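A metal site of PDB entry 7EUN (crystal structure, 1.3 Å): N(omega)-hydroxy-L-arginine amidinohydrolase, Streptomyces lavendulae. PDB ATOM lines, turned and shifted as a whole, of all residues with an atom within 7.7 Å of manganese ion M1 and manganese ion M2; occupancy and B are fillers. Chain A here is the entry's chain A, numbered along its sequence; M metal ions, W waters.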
ATOM      1  N   THR A  85      31.061  28.103 -15.007  1.00  0.00           N
ATOM      2  CA  THR A  85      30.668  28.362 -16.392  1.00  0.00           C
ATOM      3  C   THR A  85      31.001  27.160 -17.275  1.00  0.00           C
ATOM      4  O   THR A  85      31.873  26.339 -16.946  1.00  0.00           O
ATOM      5  CB  THR A  85      31.387  29.620 -16.958  1.00  0.00           C
ATOM      6  OG1 THR A  85      32.787  29.382 -16.964  1.00  0.00           O
ATOM      7  CG2 THR A  85      31.072  30.883 -16.143  1.00  0.00           C
ATOM      8  N   CYS A  86      30.345  27.103 -18.426  1.00  0.00           N
ATOM      9  CA  CYS A  86      30.683  26.085 -19.413  1.00  0.00           C
ATOM     10  C   CYS A  86      32.137  26.184 -19.852  1.00  0.00           C
ATOM     11  O   CYS A  86      32.746  25.181 -20.236  1.00  0.00           O
ATOM     12  CB  CYS A  86      29.788  26.181 -20.647  1.00  0.00           C
ATOM     13  SG  CYS A  86      28.091  25.622 -20.339  1.00  0.00           S
ATOM     14  N   SER A  87      32.736  27.387 -19.805  1.00  0.00           N
ATOM     15  CA  SER A  87      34.093  27.576 -20.300  1.00  0.00           C
ATOM     16  C   SER A  87      35.136  26.810 -19.520  1.00  0.00           C
ATOM     17  O   SER A  87      36.237  26.573 -20.045  1.00  0.00           O
ATOM     18  CB  SER A  87      34.451  29.071 -20.295  1.00  0.00           C
ATOM     19  OG  SER A  87      33.625  29.795 -21.178  1.00  0.00           O
ATOM     20  N   TYR A 107      26.452  17.182 -24.721  1.00  0.00           N
ATOM     21  CA  TYR A 107      26.610  18.605 -24.365  1.00  0.00           C
ATOM     22  C   TYR A 107      25.189  19.145 -24.288  1.00  0.00           C
ATOM     23  O   TYR A 107      24.580  19.472 -25.310  1.00  0.00           O
ATOM     24  CB  TYR A 107      27.508  19.278 -25.386  1.00  0.00           C
ATOM     25  CG  TYR A 107      28.081  20.614 -24.901  1.00  0.00           C
ATOM     26  CD1 TYR A 107      27.287  21.770 -24.889  1.00  0.00           C
ATOM     27  CD2 TYR A 107      29.398  20.730 -24.457  1.00  0.00           C
ATOM     28  CE1 TYR A 107      27.807  22.999 -24.451  1.00  0.00           C
ATOM     29  CE2 TYR A 107      29.899  21.956 -23.996  1.00  0.00           C
ATOM     30  CZ  TYR A 107      29.122  23.073 -24.025  1.00  0.00           C
ATOM     31  OH  TYR A 107      29.648  24.273 -23.565  1.00  0.00           O
ATOM     32  N   ILE A 108      24.644  19.180 -23.076  1.00  0.00           N
ATOM     33  CA  ILE A 108      23.234  19.454 -22.840  1.00  0.00           C
ATOM     34  C   ILE A 108      23.140  20.957 -22.511  1.00  0.00           C
ATOM     35  O   ILE A 108      23.648  21.412 -21.472  1.00  0.00           O
ATOM     36  CB  ILE A 108      22.678  18.575 -21.704  1.00  0.00           C
ATOM     37  CG1 ILE A 108      23.028  17.093 -21.923  1.00  0.00           C
ATOM     38  CG2 ILE A 108      21.188  18.808 -21.546  1.00  0.00           C
ATOM     39  CD1 ILE A 108      22.411  16.144 -20.906  1.00  0.00           C
ATOM     40  N   ASP A 109      22.517  21.746 -23.392  1.00  0.00           N
ATOM     41  CA  ASP A 109      22.623  23.205 -23.325  1.00  0.00           C
ATOM     42  C   ASP A 109      21.522  23.780 -24.196  1.00  0.00           C
ATOM     43  O   ASP A 109      21.193  23.218 -25.248  1.00  0.00           O
ATOM     44  CB  ASP A 109      24.017  23.598 -23.859  1.00  0.00           C
ATOM     45  CG  ASP A 109      24.458  25.027 -23.486  1.00  0.00           C
ATOM     46  OD1 ASP A 109      23.599  25.963 -23.563  1.00  0.00           O
ATOM     47  OD2 ASP A 109      25.677  25.167 -23.144  1.00  0.00           O
ATOM     48  N   GLY A 110      20.900  24.874 -23.756  1.00  0.00           N
ATOM     49  CA  GLY A 110      19.973  25.571 -24.646  1.00  0.00           C
ATOM     50  C   GLY A 110      20.615  26.205 -25.855  1.00  0.00           C
ATOM     51  O   GLY A 110      19.913  26.517 -26.835  1.00  0.00           O
ATOM     52  N   HIS A 111      21.928  26.385 -25.819  1.00  0.00           N
ATOM     53  CA  HIS A 111      22.737  26.962 -26.873  1.00  0.00           C
ATOM     54  C   HIS A 111      23.610  25.879 -27.524  1.00  0.00           C
ATOM     55  O   HIS A 111      23.770  24.786 -26.992  1.00  0.00           O
ATOM     56  CB  HIS A 111      23.677  28.032 -26.291  1.00  0.00           C
ATOM     57  CG  HIS A 111      22.991  29.137 -25.582  1.00  0.00           C
ATOM     58  ND1 HIS A 111      22.724  29.109 -24.227  1.00  0.00           N
ATOM     59  CD2 HIS A 111      22.502  30.296 -26.051  1.00  0.00           C
ATOM     60  CE1 HIS A 111      22.123  30.250 -23.894  1.00  0.00           C
ATOM     61  NE2 HIS A 111      21.971  30.975 -24.987  1.00  0.00           N
ATOM     62  N   GLY A 112      24.246  26.245 -28.634  1.00  0.00           N
ATOM     63  CA  GLY A 112      25.221  25.387 -29.262  1.00  0.00           C
ATOM     64  C   GLY A 112      26.643  25.526 -28.752  1.00  0.00           C
ATOM     65  O   GLY A 112      27.461  24.598 -28.903  1.00  0.00           O
ATOM     66  N   ASP A 113      26.966  26.686 -28.145  1.00  0.00           N
ATOM     67  CA  ASP A 113      28.309  26.975 -27.666  1.00  0.00           C
ATOM     68  C   ASP A 113      29.356  26.606 -28.711  1.00  0.00           C
ATOM     69  O   ASP A 113      30.422  26.068 -28.394  1.00  0.00           O
ATOM     70  CB  ASP A 113      28.610  26.322 -26.313  1.00  0.00           C
ATOM     71  CG  ASP A 113      27.794  26.903 -25.158  1.00  0.00           C
ATOM     72  OD1 ASP A 113      26.948  27.789 -25.394  1.00  0.00           O
ATOM     73  OD2 ASP A 113      28.028  26.475 -23.995  1.00  0.00           O
ATOM     74  N   TYR A 124      31.885  36.432 -26.216  1.00  0.00           N
ATOM     75  CA  TYR A 124      31.813  35.662 -24.973  1.00  0.00           C
ATOM     76  C   TYR A 124      32.444  34.284 -25.121  1.00  0.00           C
ATOM     77  O   TYR A 124      31.991  33.467 -25.929  1.00  0.00           O
ATOM     78  CB  TYR A 124      30.358  35.587 -24.505  1.00  0.00           C
ATOM     79  CG  TYR A 124      30.167  34.861 -23.220  1.00  0.00           C
ATOM     80  CD1 TYR A 124      31.007  35.053 -22.131  1.00  0.00           C
ATOM     81  CD2 TYR A 124      29.145  33.932 -23.106  1.00  0.00           C
ATOM     82  CE1 TYR A 124      30.820  34.346 -20.959  1.00  0.00           C
ATOM     83  CE2 TYR A 124      28.979  33.205 -21.976  1.00  0.00           C
ATOM     84  CZ  TYR A 124      29.802  33.412 -20.895  1.00  0.00           C
ATOM     85  OH  TYR A 124      29.573  32.614 -19.803  1.00  0.00           O
ATOM     86  N   GLY A 126      32.109  31.747 -23.268  1.00  0.00           N
ATOM     87  CA  GLY A 126      31.151  30.707 -22.962  1.00  0.00           C
ATOM     88  C   GLY A 126      30.342  30.270 -24.149  1.00  0.00           C
ATOM     89  O   GLY A 126      29.803  29.162 -24.139  1.00  0.00           O
ATOM     90  N   GLY A 127      30.295  31.067 -25.199  1.00  0.00           N
ATOM     91  CA  GLY A 127      29.659  30.676 -26.439  1.00  0.00           C
ATOM     92  C   GLY A 127      30.575  29.972 -27.425  1.00  0.00           C
ATOM     93  O   GLY A 127      30.148  29.707 -28.547  1.00  0.00           O
ATOM     94  N   MET A 128      31.808  29.650 -27.021  1.00  0.00           N
ATOM     95  CA  MET A 128      32.867  29.132 -27.876  1.00  0.00           C
ATOM     96  C   MET A 128      33.457  27.820 -27.348  1.00  0.00           C
ATOM     97  O   MET A 128      34.526  27.391 -27.806  1.00  0.00           O
ATOM     98  CB  MET A 128      33.985  30.193 -27.980  1.00  0.00           C
ATOM     99  CG  MET A 128      33.522  31.557 -28.506  1.00  0.00           C
ATOM    100  SD  MET A 128      34.678  32.930 -28.193  1.00  0.00           S
ATOM    101  CE  MET A 128      36.017  32.456 -29.265  1.00  0.00           C
ATOM    102  N   VAL A 129      32.780  27.190 -26.397  1.00  0.00           N
ATOM    103  CA  VAL A 129      33.395  26.091 -25.644  1.00  0.00           C
ATOM    104  C   VAL A 129      33.477  24.820 -26.483  1.00  0.00           C
ATOM    105  O   VAL A 129      34.533  24.193 -26.562  1.00  0.00           O
ATOM    106  CB  VAL A 129      32.580  25.848 -24.351  1.00  0.00           C
ATOM    107  CG1 VAL A 129      33.149  24.647 -23.596  1.00  0.00           C
ATOM    108  CG2 VAL A 129      32.573  27.082 -23.499  1.00  0.00           C
ATOM    109  N   HIS A 196      27.870  16.847 -20.009  1.00  0.00           N
ATOM    110  CA  HIS A 196      28.073  18.257 -19.678  1.00  0.00           C
ATOM    111  C   HIS A 196      26.712  18.948 -19.708  1.00  0.00           C
ATOM    112  O   HIS A 196      26.042  18.916 -20.738  1.00  0.00           O
ATOM    113  CB  HIS A 196      28.974  18.874 -20.745  1.00  0.00           C
ATOM    114  CG  HIS A 196      29.109  20.358 -20.663  1.00  0.00           C
ATOM    115  ND1 HIS A 196      30.271  20.967 -20.216  1.00  0.00           N
ATOM    116  CD2 HIS A 196      28.248  21.367 -20.946  1.00  0.00           C
ATOM    117  CE1 HIS A 196      30.106  22.279 -20.218  1.00  0.00           C
ATOM    118  NE2 HIS A 196      28.881  22.556 -20.640  1.00  0.00           N
ATOM    119  N   ILE A 197      26.300  19.591 -18.605  1.00  0.00           N
ATOM    120  CA  ILE A 197      25.021  20.290 -18.556  1.00  0.00           C
ATOM    121  C   ILE A 197      25.201  21.769 -18.217  1.00  0.00           C
ATOM    122  O   ILE A 197      25.836  22.127 -17.216  1.00  0.00           O
ATOM    123  CB  ILE A 197      24.047  19.655 -17.550  1.00  0.00           C
ATOM    124  CG1 ILE A 197      23.808  18.190 -17.792  1.00  0.00           C
ATOM    125  CG2 ILE A 197      22.706  20.358 -17.614  1.00  0.00           C
ATOM    126  CD1 ILE A 197      23.058  17.508 -16.708  1.00  0.00           C
ATOM    127  N   ASP A 198      24.589  22.622 -19.043  1.00  0.00           N
ATOM    128  CA  ASP A 198      24.354  24.049 -18.783  1.00  0.00           C
ATOM    129  C   ASP A 198      22.877  24.175 -18.427  1.00  0.00           C
ATOM    130  O   ASP A 198      22.019  23.848 -19.243  1.00  0.00           O
ATOM    131  CB  ASP A 198      24.672  24.785 -20.073  1.00  0.00           C
ATOM    132  CG  ASP A 198      24.381  26.294 -20.064  1.00  0.00           C
ATOM    133  OD1 ASP A 198      23.645  26.767 -19.184  1.00  0.00           O
ATOM    134  OD2 ASP A 198      24.854  26.982 -21.036  1.00  0.00           O
ATOM    135  N   TRP A 199      22.589  24.645 -17.206  1.00  0.00           N
ATOM    136  CA  TRP A 199      21.208  24.664 -16.753  1.00  0.00           C
ATOM    137  C   TRP A 199      20.289  25.572 -17.577  1.00  0.00           C
ATOM    138  O   TRP A 199      19.056  25.465 -17.406  1.00  0.00           O
ATOM    139  CB  TRP A 199      21.108  25.033 -15.253  1.00  0.00           C
ATOM    140  CG  TRP A 199      21.816  24.056 -14.399  1.00  0.00           C
ATOM    141  CD1 TRP A 199      22.845  24.312 -13.559  1.00  0.00           C
ATOM    142  CD2 TRP A 199      21.549  22.633 -14.288  1.00  0.00           C
ATOM    143  NE1 TRP A 199      23.265  23.154 -12.941  1.00  0.00           N
ATOM    144  CE2 TRP A 199      22.492  22.111 -13.373  1.00  0.00           C
ATOM    145  CE3 TRP A 199      20.621  21.769 -14.856  1.00  0.00           C
ATOM    146  CZ2 TRP A 199      22.521  20.775 -13.009  1.00  0.00           C
ATOM    147  CZ3 TRP A 199      20.685  20.421 -14.526  1.00  0.00           C
ATOM    148  CH2 TRP A 199      21.617  19.934 -13.602  1.00  0.00           C
ATOM    149  N   ASP A 200      20.811  26.455 -18.437  1.00  0.00           N
ATOM    150  CA  ASP A 200      19.911  27.209 -19.304  1.00  0.00           C
ATOM    151  C   ASP A 200      19.190  26.313 -20.317  1.00  0.00           C
ATOM    152  O   ASP A 200      18.301  26.801 -21.025  1.00  0.00           O
ATOM    153  CB  ASP A 200      20.557  28.424 -19.969  1.00  0.00           C
ATOM    154  CG  ASP A 200      21.643  28.112 -20.972  1.00  0.00           C
ATOM    155  OD1 ASP A 200      21.613  27.020 -21.629  1.00  0.00           O
ATOM    156  OD2 ASP A 200      22.532  28.969 -21.197  1.00  0.00           O
ATOM    157  N   VAL A 201      19.499  25.013 -20.363  1.00  0.00           N
ATOM    158  CA  VAL A 201      18.712  24.110 -21.186  1.00  0.00           C
ATOM    159  C   VAL A 201      17.280  23.983 -20.667  1.00  0.00           C
ATOM    160  O   VAL A 201      16.372  23.601 -21.432  1.00  0.00           O
ATOM    161  CB  VAL A 201      19.399  22.733 -21.291  1.00  0.00           C
ATOM    162  CG1 VAL A 201      19.266  21.943 -19.988  1.00  0.00           C
ATOM    163  CG2 VAL A 201      18.878  21.916 -22.474  1.00  0.00           C
ATOM    164  N   ALA A 240      27.010  22.908 -14.784  1.00  0.00           N
ATOM    165  CA  ALA A 240      27.474  24.285 -14.985  1.00  0.00           C
ATOM    166  C   ALA A 240      26.330  25.288 -15.084  1.00  0.00           C
ATOM    167  O   ALA A 240      25.229  24.972 -15.549  1.00  0.00           O
ATOM    168  CB  ALA A 240      28.308  24.399 -16.272  1.00  0.00           C
ATOM    169  N   GLU A 241      26.624  26.522 -14.640  1.00  0.00           N
ATOM    170  CA  GLU A 241      25.816  27.711 -14.952  1.00  0.00           C
ATOM    171  C   GLU A 241      24.505  27.747 -14.156  1.00  0.00           C
ATOM    172  O   GLU A 241      23.443  28.056 -14.689  1.00  0.00           O
ATOM    173  CB  GLU A 241      25.594  27.874 -16.462  1.00  0.00           C
ATOM    174  CG  GLU A 241      26.912  27.851 -17.220  1.00  0.00           C
ATOM    175  CD  GLU A 241      27.139  28.945 -18.252  1.00  0.00           C
ATOM    176  OE1 GLU A 241      26.224  29.731 -18.513  1.00  0.00           O
ATOM    177  OE2 GLU A 241      28.269  28.965 -18.819  1.00  0.00           O
HETATM  178 MN    MN M   1      26.778  26.721 -22.181  1.00  0.00          MN
HETATM  179 MN    MN M   2      23.606  27.799 -22.643  1.00  0.00          MN
HETATM  180  O   HOH W   1      27.843  28.601 -21.670  1.00  0.00           O
HETATM  181  O   HOH W   2      25.577  28.384 -23.278  1.00  0.00           O
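The backbone NH (N) of Cys 86 sits at hydrogen-bond distance from the side-chain carboxylate (OE2) of Glu 241 (2.8 Å). The side-chain sulfur (SG) of Cys 86 lies close to a ring nitrogen (NE2) of His 196, at 3.2 Å. The backbone carbonyl oxygen (O) of Asp 113 is in hydrogen-bond range of the backbone NH (N) of Val 129 (3.3 Å). The side-chain carboxylate of Asp 200 sits close to the backbone NH of Gly 110, at 3.1 Å. O of Ile 108 is in hydrogen-bond range of N of Asp 198 (2.9 Å). The side-chain hydroxyl of Tyr 107 lies close to the side-chain carboxylate of Asp 113, at 2.8 Å.
Of the 23 residues printed, 4 come within 4 Å of manganese ion M1. Along chain A the residues within 4 Å of manganese ion M1 span positions 86 to 198.
Within 4 Å of manganese ion M2: Asp 109, His 111, Asp 198 and Asp 200. The nearest printed residue that does not touch manganese ion M2 is Gly 110 (4.1 Å).
The side-chain carboxylate (OD2) of Asp 109 is bound to manganese ion M1, 2.1 Å away. The side-chain carboxylate (OD2) of Asp 113 binds manganese ion M1. Water W1 binds manganese ion M1, at 2.2 Å. Manganese ion M1 is bound by the side-chain carboxylate (OD2) of Asp 198 (2.3 Å). Manganese ion M1 is bound by water W2. SG of Cys 86 binds manganese ion M1 (2.5 Å).
OD1 of Asp 109 binds manganese ion M2, 2.1 Å away. Manganese ion M2 is bound by OD2 of Asp 200 (2.1 Å). Manganese ion M2 is bound by water W2 (2.2 Å). Manganese ion M2 is bound by OD2 of Asp 198, 2.2 Å away. ND1 of His 111 is bound to manganese ion M2 (2.2 Å). Manganese ion M2 is bound by the side-chain carboxylate (OD1) of Asp 200 (2.4 Å). Manganese ion M2 has six donor atoms within binding distance.
Water W1 lies within hydrogen-bond range of OE2 of Glu 241 (2.9 Å) and O of Gly 126 (3.2 Å).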
